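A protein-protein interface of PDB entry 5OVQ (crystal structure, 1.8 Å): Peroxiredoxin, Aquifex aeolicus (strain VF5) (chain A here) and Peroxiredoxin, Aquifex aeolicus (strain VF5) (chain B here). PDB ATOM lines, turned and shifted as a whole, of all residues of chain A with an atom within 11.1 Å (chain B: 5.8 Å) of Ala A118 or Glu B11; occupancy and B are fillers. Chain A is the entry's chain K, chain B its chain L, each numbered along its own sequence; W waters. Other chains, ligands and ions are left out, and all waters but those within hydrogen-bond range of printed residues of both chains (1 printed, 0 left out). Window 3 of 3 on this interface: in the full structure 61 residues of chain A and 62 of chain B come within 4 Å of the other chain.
The backbone NH of Leu B9 sits at hydrogen-bond distance from a ring nitrogen (ND1) of His A116.
Water W1 lies within hydrogen-bond range of the backbone NH (N) of Ala A118 (2.8 Å), the backbone carbonyl oxygen (O) of Leu B9 (2.8 Å) and the side-chain carboxylate (OE2) of Glu B11 (2.8 Å).
Printed residues of chain B that touch a printed residue of chain A: Arg B8, Leu B9, Gly B10 and Glu B11.
Hydrophobic or aromatic side chains of chain B that line the printed part of chain A: Leu B9.
Of the 18 printed residues of chain A, 3 touch a printed residue of chain B.
Hydrophobic or aromatic side chains of chain A that line the printed part of chain B: His A116 and Ala A118.
Along chain A the printed residues that touch a printed residue of chain B span positions 116 to 119.
Among the printed residues, 6 pairs touch across the chains.
Ile A115 touches none of the printed residues of chain B.
Printed residues of chain B within 4 Å of His A116: Arg B8 (3.5 Å) and Leu B9 (2.9 Å).
Of the printed residues of chain B, Ala A118 touches Leu B9, Gly B10 and Glu B11.
Printed residues of chain B within 4 Å of Gln A119: Leu B9 (3.8 Å).
Of the printed residues of chain A, Arg B8 touches His A116.
Gly B10 touches just one residue of chain A: Ala A118.
Of the printed residues of chain A, Glu B11 touches Ala A118.
No residue of chain A comes within 4 Å of Pro B12.
No residue of chain A comes within 4 Å of Ile B136.
His A116 touches Arg B8 (ND1 to CA, 3.5 Å).
Ala A118 touches Leu B9.
Gly B10 touches Ala A118 (O to CB, 3.6 Å).
Ala A118 touches Glu B11 (CB to CG, 3.7 Å).
Gln A119 touches Leu B9 (CG to CB, 3.8 Å).
OE1 of Gln A119 is in hydrogen-bond range of N of Leu A145 (2.9 Å).
The backbone carbonyl oxygen of Leu B137 sits at hydrogen-bond distance from the backbone NH of Gly B10 (2.8 Å).
A ring nitrogen (NE2) of His A116 sits at hydrogen-bond distance from the backbone carbonyl oxygen of Gly A113 (2.9 Å).
O of Glu B11 sits at hydrogen-bond distance from N of Leu B137, 3.0 Å away.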
ATOM      1  N   SER A   5      26.339  25.682 -13.870  1.00  0.00           N
ATOM      2  CA  SER A   5      27.159  26.836 -14.236  1.00  0.00           C
ATOM      3  C   SER A   5      26.306  27.727 -15.023  1.00  0.00           C
ATOM      4  O   SER A   5      25.454  27.298 -15.698  1.00  0.00           O
ATOM      5  CB  SER A   5      28.468  26.568 -14.951  1.00  0.00           C
ATOM      6  OG  SER A   5      29.265  27.725 -14.888  1.00  0.00           O
ATOM      7  N   GLY A 113      22.144  25.741 -17.600  1.00  0.00           N
ATOM      8  CA  GLY A 113      21.812  25.948 -16.200  1.00  0.00           C
ATOM      9  C   GLY A 113      20.334  25.869 -15.915  1.00  0.00           C
ATOM     10  O   GLY A 113      19.828  26.596 -15.052  1.00  0.00           O
ATOM     11  N   MET A 114      19.615  25.031 -16.652  1.00  0.00           N
ATOM     12  CA  MET A 114      18.170  24.990 -16.520  1.00  0.00           C
ATOM     13  C   MET A 114      17.684  24.050 -15.424  1.00  0.00           C
ATOM     14  O   MET A 114      16.500  24.109 -15.072  1.00  0.00           O
ATOM     15  CB  MET A 114      17.527  24.594 -17.847  1.00  0.00           C
ATOM     16  CG  MET A 114      17.763  25.569 -18.996  1.00  0.00           C
ATOM     17  SD  MET A 114      17.101  24.811 -20.490  1.00  0.00           S
ATOM     18  CE  MET A 114      17.360  26.014 -21.779  1.00  0.00           C
ATOM     19  N   ILE A 115      18.554  23.213 -14.860  1.00  0.00           N
ATOM     20  CA  ILE A 115      18.168  22.265 -13.819  1.00  0.00           C
ATOM     21  C   ILE A 115      18.569  22.826 -12.463  1.00  0.00           C
ATOM     22  O   ILE A 115      19.763  22.917 -12.145  1.00  0.00           O
ATOM     23  CB  ILE A 115      18.797  20.883 -14.043  1.00  0.00           C
ATOM     24  CG1 ILE A 115      18.497  20.391 -15.457  1.00  0.00           C
ATOM     25  CG2 ILE A 115      18.234  19.902 -13.037  1.00  0.00           C
ATOM     26  CD1 ILE A 115      17.012  20.211 -15.725  1.00  0.00           C
ATOM     27  N   HIS A 116      17.570  23.128 -11.640  1.00  0.00           N
ATOM     28  CA  HIS A 116      17.773  23.643 -10.287  1.00  0.00           C
ATOM     29  C   HIS A 116      17.205  22.644  -9.298  1.00  0.00           C
ATOM     30  O   HIS A 116      15.985  22.621  -9.063  1.00  0.00           O
ATOM     31  CB  HIS A 116      17.118  25.016 -10.134  1.00  0.00           C
ATOM     32  CG  HIS A 116      17.801  26.075 -10.938  1.00  0.00           C
ATOM     33  ND1 HIS A 116      18.476  27.128 -10.356  1.00  0.00           N
ATOM     34  CD2 HIS A 116      18.002  26.190 -12.273  1.00  0.00           C
ATOM     35  CE1 HIS A 116      19.018  27.874 -11.300  1.00  0.00           C
ATOM     36  NE2 HIS A 116      18.758  27.323 -12.471  1.00  0.00           N
ATOM     37  N   PRO A 117      18.051  21.827  -8.667  1.00  0.00           N
ATOM     38  CA  PRO A 117      17.549  20.618  -7.985  1.00  0.00           C
ATOM     39  C   PRO A 117      16.528  20.881  -6.898  1.00  0.00           C
ATOM     40  O   PRO A 117      15.631  20.048  -6.702  1.00  0.00           O
ATOM     41  CB  PRO A 117      18.827  19.986  -7.419  1.00  0.00           C
ATOM     42  CG  PRO A 117      19.923  20.499  -8.304  1.00  0.00           C
ATOM     43  CD  PRO A 117      19.522  21.891  -8.693  1.00  0.00           C
ATOM     44  N   ALA A 118      16.612  22.011  -6.190  1.00  0.00           N
ATOM     45  CA  ALA A 118      15.581  22.325  -5.207  1.00  0.00           C
ATOM     46  C   ALA A 118      14.243  22.643  -5.857  1.00  0.00           C
ATOM     47  O   ALA A 118      13.210  22.565  -5.183  1.00  0.00           O
ATOM     48  CB  ALA A 118      16.005  23.506  -4.329  1.00  0.00           C
ATOM     49  N   GLN A 119      14.249  23.046  -7.131  1.00  0.00           N
ATOM     50  CA  GLN A 119      13.017  23.174  -7.905  1.00  0.00           C
ATOM     51  C   GLN A 119      12.570  21.825  -8.440  1.00  0.00           C
ATOM     52  O   GLN A 119      11.432  21.398  -8.217  1.00  0.00           O
ATOM     53  CB  GLN A 119      13.235  24.135  -9.067  1.00  0.00           C
ATOM     54  CG  GLN A 119      13.306  25.583  -8.640  1.00  0.00           C
ATOM     55  CD  GLN A 119      11.925  26.178  -8.607  1.00  0.00           C
ATOM     56  OE1 GLN A 119      11.347  26.455  -9.648  1.00  0.00           O
ATOM     57  NE2 GLN A 119      11.371  26.345  -7.413  1.00  0.00           N
ATOM     58  N   SER A 120      13.460  21.158  -9.163  1.00  0.00           N
ATOM     59  CA  SER A 120      13.199  19.825  -9.687  1.00  0.00           C
ATOM     60  C   SER A 120      14.527  19.210 -10.093  1.00  0.00           C
ATOM     61  O   SER A 120      15.353  19.868 -10.730  1.00  0.00           O
ATOM     62  CB  SER A 120      12.257  19.850 -10.891  1.00  0.00           C
ATOM     63  OG  SER A 120      12.128  18.536 -11.444  1.00  0.00           O
ATOM     64  N   THR A 121      14.716  17.941  -9.746  1.00  0.00           N
ATOM     65  CA  THR A 121      15.869  17.213 -10.241  1.00  0.00           C
ATOM     66  C   THR A 121      15.597  16.567 -11.592  1.00  0.00           C
ATOM     67  O   THR A 121      16.510  15.963 -12.166  1.00  0.00           O
ATOM     68  CB  THR A 121      16.307  16.138  -9.236  1.00  0.00           C
ATOM     69  OG1 THR A 121      15.230  15.233  -8.990  1.00  0.00           O
ATOM     70  CG2 THR A 121      16.698  16.794  -7.924  1.00  0.00           C
ATOM     71  N   THR A 122      14.369  16.665 -12.100  1.00  0.00           N
ATOM     72  CA  THR A 122      13.999  16.047 -13.361  1.00  0.00           C
ATOM     73  C   THR A 122      13.501  17.025 -14.417  1.00  0.00           C
ATOM     74  O   THR A 122      13.600  16.717 -15.607  1.00  0.00           O
ATOM     75  CB  THR A 122      12.929  14.965 -13.128  1.00  0.00           C
ATOM     76  OG1 THR A 122      11.742  15.560 -12.600  1.00  0.00           O
ATOM     77  CG2 THR A 122      13.454  13.932 -12.126  1.00  0.00           C
ATOM     78  N   PHE A 123      12.942  18.170 -14.027  1.00  0.00           N
ATOM     79  CA  PHE A 123      12.375  19.127 -14.963  1.00  0.00           C
ATOM     80  C   PHE A 123      13.246  20.375 -15.006  1.00  0.00           C
ATOM     81  O   PHE A 123      13.887  20.722 -14.014  1.00  0.00           O
ATOM     82  CB  PHE A 123      10.958  19.574 -14.560  1.00  0.00           C
ATOM     83  CG  PHE A 123      10.003  18.460 -14.262  1.00  0.00           C
ATOM     84  CD1 PHE A 123       9.915  17.352 -15.080  1.00  0.00           C
ATOM     85  CD2 PHE A 123       9.139  18.563 -13.178  1.00  0.00           C
ATOM     86  CE1 PHE A 123       8.995  16.340 -14.801  1.00  0.00           C
ATOM     87  CE2 PHE A 123       8.229  17.568 -12.891  1.00  0.00           C
ATOM     88  CZ  PHE A 123       8.155  16.451 -13.702  1.00  0.00           C
ATOM     89  N   THR A 124      13.255  21.055 -16.152  1.00  0.00           N
ATOM     90  CA  THR A 124      13.847  22.390 -16.197  1.00  0.00           C
ATOM     91  C   THR A 124      12.973  23.392 -15.443  1.00  0.00           C
ATOM     92  O   THR A 124      11.771  23.197 -15.254  1.00  0.00           O
ATOM     93  CB  THR A 124      14.015  22.892 -17.635  1.00  0.00           C
ATOM     94  OG1 THR A 124      12.721  23.021 -18.258  1.00  0.00           O
ATOM     95  CG2 THR A 124      14.875  21.988 -18.446  1.00  0.00           C
ATOM     96  N   VAL A 125      13.595  24.490 -15.015  1.00  0.00           N
ATOM     97  CA  VAL A 125      12.831  25.641 -14.545  1.00  0.00           C
ATOM     98  C   VAL A 125      12.346  26.417 -15.765  1.00  0.00           C
ATOM     99  O   VAL A 125      12.457  25.936 -16.900  1.00  0.00           O
ATOM    100  CB  VAL A 125      13.663  26.533 -13.599  1.00  0.00           C
ATOM    101  CG1 VAL A 125      14.089  25.746 -12.365  1.00  0.00           C
ATOM    102  CG2 VAL A 125      14.873  27.103 -14.330  1.00  0.00           C
ATOM    103  N   TYR A 143      12.753  31.912 -14.204  1.00  0.00           N
ATOM    104  CA  TYR A 143      11.597  31.969 -13.328  1.00  0.00           C
ATOM    105  C   TYR A 143      11.300  30.584 -12.761  1.00  0.00           C
ATOM    106  O   TYR A 143      11.653  29.576 -13.372  1.00  0.00           O
ATOM    107  CB  TYR A 143      10.366  32.489 -14.084  1.00  0.00           C
ATOM    108  CG  TYR A 143      10.255  33.997 -14.231  1.00  0.00           C
ATOM    109  CD1 TYR A 143      11.360  34.833 -14.051  1.00  0.00           C
ATOM    110  CD2 TYR A 143       9.035  34.587 -14.554  1.00  0.00           C
ATOM    111  CE1 TYR A 143      11.240  36.219 -14.189  1.00  0.00           C
ATOM    112  CE2 TYR A 143       8.908  35.976 -14.691  1.00  0.00           C
ATOM    113  CZ  TYR A 143      10.017  36.782 -14.510  1.00  0.00           C
ATOM    114  OH  TYR A 143       9.895  38.152 -14.650  1.00  0.00           O
ATOM    115  N   PRO A 144      10.671  30.492 -11.593  1.00  0.00           N
ATOM    116  CA  PRO A 144      10.435  29.190 -10.959  1.00  0.00           C
ATOM    117  C   PRO A 144       9.200  28.482 -11.528  1.00  0.00           C
ATOM    118  O   PRO A 144       8.422  29.032 -12.313  1.00  0.00           O
ATOM    119  CB  PRO A 144      10.237  29.567  -9.490  1.00  0.00           C
ATOM    120  CG  PRO A 144       9.591  30.947  -9.566  1.00  0.00           C
ATOM    121  CD  PRO A 144      10.269  31.619 -10.726  1.00  0.00           C
ATOM    122  N   LEU A 145       8.999  27.245 -11.064  1.00  0.00           N
ATOM    123  CA  LEU A 145       7.916  26.418 -11.594  1.00  0.00           C
ATOM    124  C   LEU A 145       6.547  27.057 -11.386  1.00  0.00           C
ATOM    125  O   LEU A 145       5.636  26.861 -12.203  1.00  0.00           O
ATOM    126  CB  LEU A 145       7.944  25.043 -10.928  1.00  0.00           C
ATOM    127  CG  LEU A 145       9.236  24.234 -11.027  1.00  0.00           C
ATOM    128  CD1 LEU A 145       9.060  22.909 -10.311  1.00  0.00           C
ATOM    129  CD2 LEU A 145       9.664  24.029 -12.478  1.00  0.00           C
ATOM    130  N   THR A 146       6.379  27.815 -10.302  1.00  0.00           N
ATOM    131  CA  THR A 146       5.081  28.396  -9.977  1.00  0.00           C
ATOM    132  C   THR A 146       4.647  29.513 -10.920  1.00  0.00           C
ATOM    133  O   THR A 146       3.451  29.803 -10.986  1.00  0.00           O
ATOM    134  CB  THR A 146       5.090  28.965  -8.551  1.00  0.00           C
ATOM    135  OG1 THR A 146       6.223  29.842  -8.391  1.00  0.00           O
ATOM    136  CG2 THR A 146       5.154  27.848  -7.521  1.00  0.00           C
ATOM    137  N   ARG B   8      21.295  29.113  -7.320  1.00  0.00           N
ATOM    138  CA  ARG B   8      20.344  28.028  -7.481  1.00  0.00           C
ATOM    139  C   ARG B   8      18.968  28.423  -6.954  1.00  0.00           C
ATOM    140  O   ARG B   8      18.816  28.757  -5.776  1.00  0.00           O
ATOM    141  CB  ARG B   8      20.863  26.751  -6.814  1.00  0.00           C
ATOM    142  CG  ARG B   8      22.061  26.139  -7.560  1.00  0.00           C
ATOM    143  CD  ARG B   8      22.591  24.899  -6.902  1.00  0.00           C
ATOM    144  NE  ARG B   8      23.595  24.229  -7.732  1.00  0.00           N
ATOM    145  CZ  ARG B   8      24.886  24.561  -7.787  1.00  0.00           C
ATOM    146  NH1 ARG B   8      25.341  25.572  -7.071  1.00  0.00           N
ATOM    147  NH2 ARG B   8      25.692  23.893  -8.594  1.00  0.00           N
ATOM    148  N   LEU B   9      17.966  28.351  -7.828  1.00  0.00           N
ATOM    149  CA  LEU B   9      16.595  28.628  -7.423  1.00  0.00           C
ATOM    150  C   LEU B   9      16.132  27.607  -6.391  1.00  0.00           C
ATOM    151  O   LEU B   9      16.446  26.414  -6.482  1.00  0.00           O
ATOM    152  CB  LEU B   9      15.679  28.604  -8.644  1.00  0.00           C
ATOM    153  CG  LEU B   9      15.944  29.644  -9.736  1.00  0.00           C
ATOM    154  CD1 LEU B   9      14.910  29.503 -10.861  1.00  0.00           C
ATOM    155  CD2 LEU B   9      15.921  31.059  -9.167  1.00  0.00           C
ATOM    156  N   GLY B  10      15.418  28.092  -5.383  1.00  0.00           N
ATOM    157  CA  GLY B  10      14.895  27.253  -4.333  1.00  0.00           C
ATOM    158  C   GLY B  10      15.829  26.984  -3.172  1.00  0.00           C
ATOM    159  O   GLY B  10      15.414  26.316  -2.218  1.00  0.00           O
ATOM    160  N   GLU B  11      17.071  27.466  -3.213  1.00  0.00           N
ATOM    161  CA  GLU B  11      18.021  27.279  -2.134  1.00  0.00           C
ATOM    162  C   GLU B  11      18.290  28.609  -1.449  1.00  0.00           C
ATOM    163  O   GLU B  11      18.023  29.669  -2.026  1.00  0.00           O
ATOM    164  CB  GLU B  11      19.319  26.669  -2.682  1.00  0.00           C
ATOM    165  CG  GLU B  11      19.033  25.408  -3.513  1.00  0.00           C
ATOM    166  CD  GLU B  11      20.265  24.593  -3.879  1.00  0.00           C
ATOM    167  OE1 GLU B  11      21.305  24.695  -3.198  1.00  0.00           O
ATOM    168  OE2 GLU B  11      20.176  23.827  -4.861  1.00  0.00           O
ATOM    169  N   PRO B  12      18.784  28.597  -0.206  1.00  0.00           N
ATOM    170  CA  PRO B  12      19.087  29.865   0.466  1.00  0.00           C
ATOM    171  C   PRO B  12      19.937  30.757  -0.421  1.00  0.00           C
ATOM    172  O   PRO B  12      20.859  30.294  -1.095  1.00  0.00           O
ATOM    173  CB  PRO B  12      19.841  29.428   1.725  1.00  0.00           C
ATOM    174  CG  PRO B  12      19.267  28.070   2.020  1.00  0.00           C
ATOM    175  CD  PRO B  12      18.992  27.439   0.687  1.00  0.00           C
ATOM    176  N   ALA B  13      19.590  32.041  -0.446  1.00  0.00           N
ATOM    177  CA  ALA B  13      20.373  32.995  -1.207  1.00  0.00           C
ATOM    178  C   ALA B  13      21.785  33.063  -0.632  1.00  0.00           C
ATOM    179  O   ALA B  13      21.956  33.023   0.594  1.00  0.00           O
ATOM    180  CB  ALA B  13      19.727  34.378  -1.166  1.00  0.00           C
ATOM    181  N   GLY B 135      14.574  33.837   3.131  1.00  0.00           N
ATOM    182  CA  GLY B 135      15.912  33.899   2.584  1.00  0.00           C
ATOM    183  C   GLY B 135      16.151  32.985   1.405  1.00  0.00           C
ATOM    184  O   GLY B 135      17.311  32.775   1.028  1.00  0.00           O
ATOM    185  N   ILE B 136      15.096  32.428   0.816  1.00  0.00           N
ATOM    186  CA  ILE B 136      15.222  31.502  -0.302  1.00  0.00           C
ATOM    187  C   ILE B 136      15.188  32.280  -1.608  1.00  0.00           C
ATOM    188  O   ILE B 136      14.315  33.132  -1.816  1.00  0.00           O
ATOM    189  CB  ILE B 136      14.104  30.446  -0.270  1.00  0.00           C
ATOM    190  CG1 ILE B 136      14.205  29.602   1.004  1.00  0.00           C
ATOM    191  CG2 ILE B 136      14.152  29.586  -1.518  1.00  0.00           C
ATOM    192  CD1 ILE B 136      15.467  28.774   1.082  1.00  0.00           C
ATOM    193  N   LEU B 137      16.126  31.967  -2.495  1.00  0.00           N
ATOM    194  CA  LEU B 137      16.125  32.530  -3.838  1.00  0.00           C
ATOM    195  C   LEU B 137      14.960  31.974  -4.651  1.00  0.00           C
ATOM    196  O   LEU B 137      14.769  30.759  -4.727  1.00  0.00           O
ATOM    197  CB  LEU B 137      17.437  32.205  -4.529  1.00  0.00           C
ATOM    198  CG  LEU B 137      17.558  32.662  -5.967  1.00  0.00           C
ATOM    199  CD1 LEU B 137      17.417  34.190  -6.041  1.00  0.00           C
ATOM    200  CD2 LEU B 137      18.924  32.230  -6.371  1.00  0.00           C
HETATM  201  O   HOH W   1      18.201  24.239  -6.863  1.00  0.00           O
